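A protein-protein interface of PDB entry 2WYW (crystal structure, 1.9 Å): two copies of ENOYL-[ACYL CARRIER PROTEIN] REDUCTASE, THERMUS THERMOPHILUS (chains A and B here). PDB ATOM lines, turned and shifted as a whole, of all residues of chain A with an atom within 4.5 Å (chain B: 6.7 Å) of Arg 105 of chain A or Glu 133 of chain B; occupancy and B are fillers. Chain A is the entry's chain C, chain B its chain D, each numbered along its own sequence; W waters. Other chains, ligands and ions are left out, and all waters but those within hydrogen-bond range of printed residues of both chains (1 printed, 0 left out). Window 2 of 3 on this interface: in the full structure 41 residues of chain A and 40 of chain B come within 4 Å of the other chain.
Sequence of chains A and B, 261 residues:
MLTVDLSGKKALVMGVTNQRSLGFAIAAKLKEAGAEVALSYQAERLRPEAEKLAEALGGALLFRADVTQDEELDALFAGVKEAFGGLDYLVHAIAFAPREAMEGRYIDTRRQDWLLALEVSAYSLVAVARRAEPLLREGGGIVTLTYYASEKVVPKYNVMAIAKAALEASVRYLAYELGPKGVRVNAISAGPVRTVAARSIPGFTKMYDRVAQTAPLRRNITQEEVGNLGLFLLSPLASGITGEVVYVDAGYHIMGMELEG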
ATOM      1  N   ALA A 101      -5.657  16.534 -22.604  1.00  0.00           N
ATOM      2  CA  ALA A 101      -6.533  17.488 -21.905  1.00  0.00           C
ATOM      3  C   ALA A 101      -6.026  18.921 -22.013  1.00  0.00           C
ATOM      4  O   ALA A 101      -6.819  19.867 -22.157  1.00  0.00           O
ATOM      5  CB  ALA A 101      -6.678  17.086 -20.444  1.00  0.00           C
ATOM      6  N   GLY A 104      -6.074  20.309 -25.975  1.00  0.00           N
ATOM      7  CA  GLY A 104      -7.371  20.601 -26.598  1.00  0.00           C
ATOM      8  C   GLY A 104      -8.083  21.808 -25.995  1.00  0.00           C
ATOM      9  O   GLY A 104      -7.440  22.750 -25.517  1.00  0.00           O
ATOM     10  N   ARG A 105      -9.417  21.802 -26.078  1.00  0.00           N
ATOM     11  CA  ARG A 105     -10.264  22.748 -25.334  1.00  0.00           C
ATOM     12  C   ARG A 105     -10.688  22.062 -24.051  1.00  0.00           C
ATOM     13  O   ARG A 105     -10.688  20.835 -23.989  1.00  0.00           O
ATOM     14  CB  ARG A 105     -11.510  23.111 -26.144  1.00  0.00           C
ATOM     15  CG  ARG A 105     -11.195  23.798 -27.495  1.00  0.00           C
ATOM     16  CD  ARG A 105     -12.475  24.203 -28.208  1.00  0.00           C
ATOM     17  NE  ARG A 105     -13.347  23.052 -28.415  1.00  0.00           N
ATOM     18  CZ  ARG A 105     -14.647  23.120 -28.676  1.00  0.00           C
ATOM     19  NH1 ARG A 105     -15.255  24.283 -28.807  1.00  0.00           N
ATOM     20  NH2 ARG A 105     -15.338  22.012 -28.819  1.00  0.00           N
ATOM     21  N   TYR A 106     -11.050  22.849 -23.030  1.00  0.00           N
ATOM     22  CA  TYR A 106     -11.588  22.303 -21.781  1.00  0.00           C
ATOM     23  C   TYR A 106     -12.865  21.471 -22.010  1.00  0.00           C
ATOM     24  O   TYR A 106     -13.026  20.370 -21.459  1.00  0.00           O
ATOM     25  CB  TYR A 106     -11.842  23.436 -20.756  1.00  0.00           C
ATOM     26  CG  TYR A 106     -12.464  22.895 -19.500  1.00  0.00           C
ATOM     27  CD1 TYR A 106     -11.778  21.962 -18.730  1.00  0.00           C
ATOM     28  CD2 TYR A 106     -13.739  23.269 -19.105  1.00  0.00           C
ATOM     29  CE1 TYR A 106     -12.332  21.421 -17.594  1.00  0.00           C
ATOM     30  CE2 TYR A 106     -14.327  22.717 -17.964  1.00  0.00           C
ATOM     31  CZ  TYR A 106     -13.604  21.797 -17.210  1.00  0.00           C
ATOM     32  OH  TYR A 106     -14.137  21.214 -16.101  1.00  0.00           O
ATOM     33  N   ILE A 107     -13.745  21.999 -22.860  1.00  0.00           N
ATOM     34  CA  ILE A 107     -15.026  21.389 -23.185  1.00  0.00           C
ATOM     35  C   ILE A 107     -14.867  19.985 -23.812  1.00  0.00           C
ATOM     36  O   ILE A 107     -15.777  19.170 -23.744  1.00  0.00           O
ATOM     37  CB  ILE A 107     -15.831  22.310 -24.157  1.00  0.00           C
ATOM     38  CG1 ILE A 107     -17.308  21.878 -24.240  1.00  0.00           C
ATOM     39  CG2 ILE A 107     -15.166  22.359 -25.552  1.00  0.00           C
ATOM     40  CD1 ILE A 107     -18.243  22.985 -24.745  1.00  0.00           C
ATOM     41  N   ASP A 108     -13.697  19.722 -24.390  1.00  0.00           N
ATOM     42  CA  ASP A 108     -13.397  18.451 -25.059  1.00  0.00           C
ATOM     43  C   ASP A 108     -12.652  17.452 -24.196  1.00  0.00           C
ATOM     44  O   ASP A 108     -12.283  16.371 -24.682  1.00  0.00           O
ATOM     45  CB  ASP A 108     -12.596  18.733 -26.336  1.00  0.00           C
ATOM     46  CG  ASP A 108     -13.434  19.409 -27.397  1.00  0.00           C
ATOM     47  OD1 ASP A 108     -14.667  19.195 -27.395  1.00  0.00           O
ATOM     48  OD2 ASP A 108     -12.861  20.156 -28.214  1.00  0.00           O
ATOM     49  N   THR A 109     -12.445  17.797 -22.918  1.00  0.00           N
ATOM     50  CA  THR A 109     -11.745  16.909 -21.993  1.00  0.00           C
ATOM     51  C   THR A 109     -12.485  15.579 -21.833  1.00  0.00           C
ATOM     52  O   THR A 109     -13.675  15.560 -21.513  1.00  0.00           O
ATOM     53  CB  THR A 109     -11.583  17.535 -20.578  1.00  0.00           C
ATOM     54  OG1 THR A 109     -11.242  18.917 -20.700  1.00  0.00           O
ATOM     55  CG2 THR A 109     -10.519  16.782 -19.777  1.00  0.00           C
ATOM     56  N   LYS A 156      -5.797  27.335 -22.355  1.00  0.00           N
ATOM     57  CA  LYS A 156      -4.860  26.187 -22.390  1.00  0.00           C
ATOM     58  C   LYS A 156      -4.423  25.624 -21.040  1.00  0.00           C
ATOM     59  O   LYS A 156      -3.837  24.549 -21.017  1.00  0.00           O
ATOM     60  CB  LYS A 156      -3.626  26.466 -23.277  1.00  0.00           C
ATOM     61  CG  LYS A 156      -3.923  26.580 -24.788  1.00  0.00           C
ATOM     62  CD  LYS A 156      -4.597  25.297 -25.348  1.00  0.00           C
ATOM     63  CE  LYS A 156      -4.937  25.433 -26.836  1.00  0.00           C
ATOM     64  NZ  LYS A 156      -6.156  24.647 -27.226  1.00  0.00           N
ATOM     65  N   ASN A 158      -6.809  24.938 -18.943  1.00  0.00           N
ATOM     66  CA  ASN A 158      -7.888  23.958 -19.111  1.00  0.00           C
ATOM     67  C   ASN A 158      -8.243  23.219 -17.811  1.00  0.00           C
ATOM     68  O   ASN A 158      -8.444  23.878 -16.797  1.00  0.00           O
ATOM     69  CB  ASN A 158      -7.540  23.001 -20.263  1.00  0.00           C
ATOM     70  CG  ASN A 158      -7.553  23.685 -21.606  1.00  0.00           C
ATOM     71  OD1 ASN A 158      -7.941  24.836 -21.708  1.00  0.00           O
ATOM     72  ND2 ASN A 158      -7.164  22.961 -22.664  1.00  0.00           N
ATOM     73  N   PHE B  77     -28.726  13.185 -26.346  1.00  0.00           N
ATOM     74  CA  PHE B  77     -28.573  14.308 -27.252  1.00  0.00           C
ATOM     75  C   PHE B  77     -28.968  13.967 -28.665  1.00  0.00           C
ATOM     76  O   PHE B  77     -29.489  14.829 -29.385  1.00  0.00           O
ATOM     77  CB  PHE B  77     -27.188  14.929 -27.126  1.00  0.00           C
ATOM     78  CG  PHE B  77     -27.084  15.806 -25.932  1.00  0.00           C
ATOM     79  CD1 PHE B  77     -27.500  17.133 -26.004  1.00  0.00           C
ATOM     80  CD2 PHE B  77     -26.689  15.280 -24.699  1.00  0.00           C
ATOM     81  CE1 PHE B  77     -27.469  17.946 -24.870  1.00  0.00           C
ATOM     82  CE2 PHE B  77     -26.639  16.077 -23.554  1.00  0.00           C
ATOM     83  CZ  PHE B  77     -27.029  17.418 -23.635  1.00  0.00           C
ATOM     84  N   VAL B 128     -22.123  17.213 -20.766  1.00  0.00           N
ATOM     85  CA  VAL B 128     -23.353  17.696 -21.400  1.00  0.00           C
ATOM     86  C   VAL B 128     -23.135  18.931 -22.271  1.00  0.00           C
ATOM     87  O   VAL B 128     -23.782  19.053 -23.341  1.00  0.00           O
ATOM     88  CB  VAL B 128     -24.506  17.894 -20.381  1.00  0.00           C
ATOM     89  CG1 VAL B 128     -24.776  16.559 -19.664  1.00  0.00           C
ATOM     90  CG2 VAL B 128     -24.204  18.988 -19.377  1.00  0.00           C
ATOM     91  N   ALA B 129     -22.223  19.827 -21.846  1.00  0.00           N
ATOM     92  CA  ALA B 129     -21.841  20.985 -22.662  1.00  0.00           C
ATOM     93  C   ALA B 129     -21.231  20.548 -23.997  1.00  0.00           C
ATOM     94  O   ALA B 129     -21.504  21.141 -25.031  1.00  0.00           O
ATOM     95  CB  ALA B 129     -20.858  21.889 -21.926  1.00  0.00           C
ATOM     96  N   ARG B 130     -20.368  19.538 -23.966  1.00  0.00           N
ATOM     97  CA  ARG B 130     -19.726  19.068 -25.203  1.00  0.00           C
ATOM     98  C   ARG B 130     -20.756  18.577 -26.234  1.00  0.00           C
ATOM     99  O   ARG B 130     -20.657  18.900 -27.417  1.00  0.00           O
ATOM    100  CB  ARG B 130     -18.717  17.961 -24.903  1.00  0.00           C
ATOM    101  CG  ARG B 130     -17.936  17.511 -26.126  1.00  0.00           C
ATOM    102  CD  ARG B 130     -16.621  16.868 -25.767  1.00  0.00           C
ATOM    103  NE  ARG B 130     -16.759  15.619 -25.021  1.00  0.00           N
ATOM    104  CZ  ARG B 130     -16.393  15.453 -23.754  1.00  0.00           C
ATOM    105  NH1 ARG B 130     -15.871  16.466 -23.056  1.00  0.00           N
ATOM    106  NH2 ARG B 130     -16.549  14.264 -23.188  1.00  0.00           N
ATOM    107  N   ARG B 131     -21.708  17.790 -25.759  1.00  0.00           N
ATOM    108  CA  ARG B 131     -22.722  17.171 -26.590  1.00  0.00           C
ATOM    109  C   ARG B 131     -23.770  18.183 -27.019  1.00  0.00           C
ATOM    110  O   ARG B 131     -24.397  18.026 -28.059  1.00  0.00           O
ATOM    111  CB  ARG B 131     -23.384  16.017 -25.825  1.00  0.00           C
ATOM    112  CG  ARG B 131     -22.412  14.857 -25.562  1.00  0.00           C
ATOM    113  CD  ARG B 131     -22.983  13.844 -24.597  1.00  0.00           C
ATOM    114  NE  ARG B 131     -22.208  12.609 -24.611  1.00  0.00           N
ATOM    115  CZ  ARG B 131     -21.065  12.397 -23.955  1.00  0.00           C
ATOM    116  NH1 ARG B 131     -20.509  13.341 -23.189  1.00  0.00           N
ATOM    117  NH2 ARG B 131     -20.452  11.218 -24.066  1.00  0.00           N
ATOM    118  N   ALA B 132     -23.972  19.222 -26.207  1.00  0.00           N
ATOM    119  CA  ALA B 132     -24.951  20.245 -26.523  1.00  0.00           C
ATOM    120  C   ALA B 132     -24.403  21.213 -27.539  1.00  0.00           C
ATOM    121  O   ALA B 132     -25.155  21.726 -28.357  1.00  0.00           O
ATOM    122  CB  ALA B 132     -25.384  20.986 -25.253  1.00  0.00           C
ATOM    123  N   GLU B 133     -23.092  21.450 -27.509  1.00  0.00           N
ATOM    124  CA  GLU B 133     -22.460  22.468 -28.357  1.00  0.00           C
ATOM    125  C   GLU B 133     -22.931  22.501 -29.810  1.00  0.00           C
ATOM    126  O   GLU B 133     -23.284  23.565 -30.305  1.00  0.00           O
ATOM    127  CB  GLU B 133     -20.939  22.324 -28.340  1.00  0.00           C
ATOM    128  CG  GLU B 133     -20.203  23.395 -29.132  1.00  0.00           C
ATOM    129  CD  GLU B 133     -18.717  23.260 -29.022  1.00  0.00           C
ATOM    130  OE1 GLU B 133     -18.243  22.193 -28.582  1.00  0.00           O
ATOM    131  OE2 GLU B 133     -18.018  24.217 -29.356  1.00  0.00           O
ATOM    132  N   PRO B 134     -22.908  21.354 -30.512  1.00  0.00           N
ATOM    133  CA  PRO B 134     -23.249  21.441 -31.933  1.00  0.00           C
ATOM    134  C   PRO B 134     -24.739  21.679 -32.164  1.00  0.00           C
ATOM    135  O   PRO B 134     -25.110  22.150 -33.222  1.00  0.00           O
ATOM    136  CB  PRO B 134     -22.787  20.092 -32.492  1.00  0.00           C
ATOM    137  CG  PRO B 134     -22.897  19.162 -31.354  1.00  0.00           C
ATOM    138  CD  PRO B 134     -22.514  19.986 -30.133  1.00  0.00           C
ATOM    139  N   LEU B 135     -25.571  21.412 -31.159  1.00  0.00           N
ATOM    140  CA  LEU B 135     -27.005  21.677 -31.265  1.00  0.00           C
ATOM    141  C   LEU B 135     -27.375  23.115 -30.932  1.00  0.00           C
ATOM    142  O   LEU B 135     -28.447  23.589 -31.328  1.00  0.00           O
ATOM    143  CB  LEU B 135     -27.772  20.767 -30.325  1.00  0.00           C
ATOM    144  CG  LEU B 135     -27.912  19.303 -30.725  1.00  0.00           C
ATOM    145  CD1 LEU B 135     -26.636  18.785 -31.379  1.00  0.00           C
ATOM    146  CD2 LEU B 135     -28.304  18.487 -29.513  1.00  0.00           C
ATOM    147  N   LEU B 136     -26.514  23.790 -30.165  1.00  0.00           N
ATOM    148  CA  LEU B 136     -26.876  25.050 -29.498  1.00  0.00           C
ATOM    149  C   LEU B 136     -26.834  26.201 -30.459  1.00  0.00           C
ATOM    150  O   LEU B 136     -25.814  26.446 -31.107  1.00  0.00           O
ATOM    151  CB  LEU B 136     -25.953  25.348 -28.291  1.00  0.00           C
ATOM    152  CG  LEU B 136     -26.262  24.632 -26.962  1.00  0.00           C
ATOM    153  CD1 LEU B 136     -25.088  24.807 -25.970  1.00  0.00           C
ATOM    154  CD2 LEU B 136     -27.555  25.123 -26.332  1.00  0.00           C
ATOM    155  N   ARG B 137     -27.955  26.916 -30.538  1.00  0.00           N
ATOM    156  CA  ARG B 137     -28.106  28.042 -31.458  1.00  0.00           C
ATOM    157  C   ARG B 137     -27.486  29.327 -30.885  1.00  0.00           C
ATOM    158  O   ARG B 137     -27.422  29.499 -29.659  1.00  0.00           O
ATOM    159  CB  ARG B 137     -29.597  28.240 -31.769  1.00  0.00           C
ATOM    160  CG  ARG B 137     -30.265  27.027 -32.481  1.00  0.00           C
ATOM    161  CD  ARG B 137     -31.765  26.907 -32.135  1.00  0.00           C
ATOM    162  NE  ARG B 137     -32.411  25.735 -32.726  1.00  0.00           N
ATOM    163  CZ  ARG B 137     -33.643  25.309 -32.432  1.00  0.00           C
ATOM    164  NH1 ARG B 137     -34.400  25.951 -31.540  1.00  0.00           N
ATOM    165  NH2 ARG B 137     -34.133  24.229 -33.040  1.00  0.00           N
ATOM    166  N   ILE B 142     -26.398  27.825 -21.348  1.00  0.00           N
ATOM    167  CA  ILE B 142     -26.354  26.758 -20.352  1.00  0.00           C
ATOM    168  C   ILE B 142     -26.366  27.414 -18.973  1.00  0.00           C
ATOM    169  O   ILE B 142     -25.603  28.360 -18.696  1.00  0.00           O
ATOM    170  CB  ILE B 142     -25.072  25.887 -20.478  1.00  0.00           C
ATOM    171  CG1 ILE B 142     -24.914  25.280 -21.900  1.00  0.00           C
ATOM    172  CG2 ILE B 142     -25.086  24.746 -19.447  1.00  0.00           C
ATOM    173  CD1 ILE B 142     -23.543  24.616 -22.175  1.00  0.00           C
ATOM    174  N   GLU B 177     -15.141  29.303 -23.857  1.00  0.00           N
ATOM    175  CA  GLU B 177     -15.027  28.441 -25.028  1.00  0.00           C
ATOM    176  C   GLU B 177     -16.263  28.461 -25.911  1.00  0.00           C
ATOM    177  O   GLU B 177     -16.157  28.269 -27.127  1.00  0.00           O
ATOM    178  CB  GLU B 177     -14.659  27.039 -24.611  1.00  0.00           C
ATOM    179  CG  GLU B 177     -13.233  26.999 -24.083  1.00  0.00           C
ATOM    180  CD  GLU B 177     -12.756  25.601 -23.794  1.00  0.00           C
ATOM    181  OE1 GLU B 177     -13.612  24.706 -23.713  1.00  0.00           O
ATOM    182  OE2 GLU B 177     -11.539  25.412 -23.617  1.00  0.00           O
ATOM    183  N   LEU B 178     -17.430  28.717 -25.323  1.00  0.00           N
ATOM    184  CA  LEU B 178     -18.674  28.784 -26.100  1.00  0.00           C
ATOM    185  C   LEU B 178     -19.064  30.200 -26.501  1.00  0.00           C
ATOM    186  O   LEU B 178     -19.911  30.380 -27.362  1.00  0.00           O
ATOM    187  CB  LEU B 178     -19.809  28.143 -25.314  1.00  0.00           C
ATOM    188  CG  LEU B 178     -19.691  26.623 -25.187  1.00  0.00           C
ATOM    189  CD1 LEU B 178     -20.698  26.114 -24.221  1.00  0.00           C
ATOM    190  CD2 LEU B 178     -19.903  25.966 -26.583  1.00  0.00           C
ATOM    191  N   LYS B 181     -19.409  31.550 -30.238  1.00  0.00           N
ATOM    192  CA  LYS B 181     -20.586  31.233 -30.999  1.00  0.00           C
ATOM    193  C   LYS B 181     -21.881  31.919 -30.521  1.00  0.00           C
ATOM    194  O   LYS B 181     -22.938  31.678 -31.062  1.00  0.00           O
ATOM    195  CB  LYS B 181     -20.733  29.722 -31.134  1.00  0.00           C
ATOM    196  CG  LYS B 181     -21.043  28.953 -29.928  1.00  0.00           C
ATOM    197  CD  LYS B 181     -21.161  27.464 -30.292  1.00  0.00           C
ATOM    198  CE  LYS B 181     -22.512  27.167 -30.930  1.00  0.00           C
ATOM    199  NZ  LYS B 181     -22.594  25.766 -31.443  1.00  0.00           N
ATOM    200  N   VAL B 183     -23.080  31.733 -27.359  1.00  0.00           N
ATOM    201  CA  VAL B 183     -23.703  30.853 -26.385  1.00  0.00           C
ATOM    202  C   VAL B 183     -23.120  31.251 -25.016  1.00  0.00           C
ATOM    203  O   VAL B 183     -21.915  31.479 -24.894  1.00  0.00           O
ATOM    204  CB  VAL B 183     -23.449  29.373 -26.698  1.00  0.00           C
ATOM    205  CG1 VAL B 183     -23.938  28.458 -25.545  1.00  0.00           C
ATOM    206  CG2 VAL B 183     -24.134  28.989 -28.044  1.00  0.00           C
HETATM  207  O   HOH W   1     -14.223  26.988 -28.373  1.00  0.00           O
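Hydrophobic or aromatic side chains of chain A within 4 Å of the printed part of chain B: Tyr 106 and Ile 107. Among the printed residues, Asp or Glu carboxylates within 4 Å of a Lys or Arg side-chain nitrogen of the other chain: Arg 105 of chain A with Glu 133 of chain B (2.8 Å).
Water W1 lies within hydrogen-bond range of the backbone carbonyl oxygen of Glu 177 of chain B (2.6 Å) and the guanidinium group of Arg 105 of chain A (2.9 Å).
Arg 105 of chain A touches Glu 177 of chain B (CA to OE2, 3.4 Å). CD1 of Ile 107 of chain A touches O of Ala 129 of chain B, at 3.8 Å. CD1 of Ile 107 of chain A touches OE1 of Glu 133 of chain B (3.9 Å). Ile 107 of chain A touches Leu 178 of chain B. CD of Arg 130 of chain B touches OD1 of Asp 108 of chain A (3.4 Å).
Of chain B, only Glu 133 and Glu 177 come within 4 Å of Arg 105 of chain A. Glu 133 of chain B touches just these residues of chain A: Arg 105 and Ile 107. Of the printed residues of chain A, Glu 177 of chain B touches Arg 105 (3.4 Å), Tyr 106 (2.7 Å) and Ile 107 (2.8 Å). Of the printed residues of chain B, Tyr 106 of chain A touches Glu 177. Of the printed residues of chain A, Leu 178 of chain B touches Ile 107. Of the printed residues of chain B, Ile 107 of chain A touches Ala 129, Arg 130, Glu 133, Glu 177 and Leu 178. Of the printed residues of chain A, Arg 130 of chain B touches Ile 107, Asp 108 and Thr 109. Gly 104 of chain A touches none of the printed residues of chain B. Phe 77 of chain B touches none of the printed residues of chain A. The nearest printed residue of chain A that does not touch Glu 133 of chain B is Asp 108 of chain A (4.8 Å).
No position is printed for both chains. Of the 10 pairs that touch across the chains among the printed residues, none has its exchanged pair printed and touching as well.
The backbone NH (N) of Tyr 106 of chain A is in hydrogen-bond range of the side-chain carboxylate (OE2) of Glu 177 of chain B, 2.7 Å away. The backbone carbonyl oxygen of Thr 109 of chain A is in hydrogen-bond range of the guanidinium group of Arg 130 of chain B, 2.8 Å away. The side-chain carboxylate (OE2) of Glu 133 of chain B is in salt-bridge range of the guanidinium group (NH1) of Arg 105 of chain A (2.8 Å). The backbone NH (N) of Ile 107 of chain A lies within hydrogen-bond range of the side-chain carboxylate (OE1) of Glu 177 of chain B (2.8 Å). The backbone carbonyl oxygen (O) of Ile 107 of chain A lies within hydrogen-bond range of the guanidinium group (NH1) of Arg 130 of chain B.
The backbone carbonyl oxygen (O) of Glu 133 of chain B sits at hydrogen-bond distance from the side-chain amino group (NZ) of Lys 181 of chain B. The backbone carbonyl oxygen (O) of Tyr 106 of chain A is in hydrogen-bond range of the side-chain hydroxyl (OG1) of Thr 109 of chain A (2.4 Å). NE of Arg 105 of chain A lies within salt-bridge range of OD2 of Asp 108 of chain A (2.9 Å). The backbone carbonyl oxygen of Leu 178 of chain B is in hydrogen-bond range of the backbone NH of Val 183 of chain B, 3.4 Å away.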
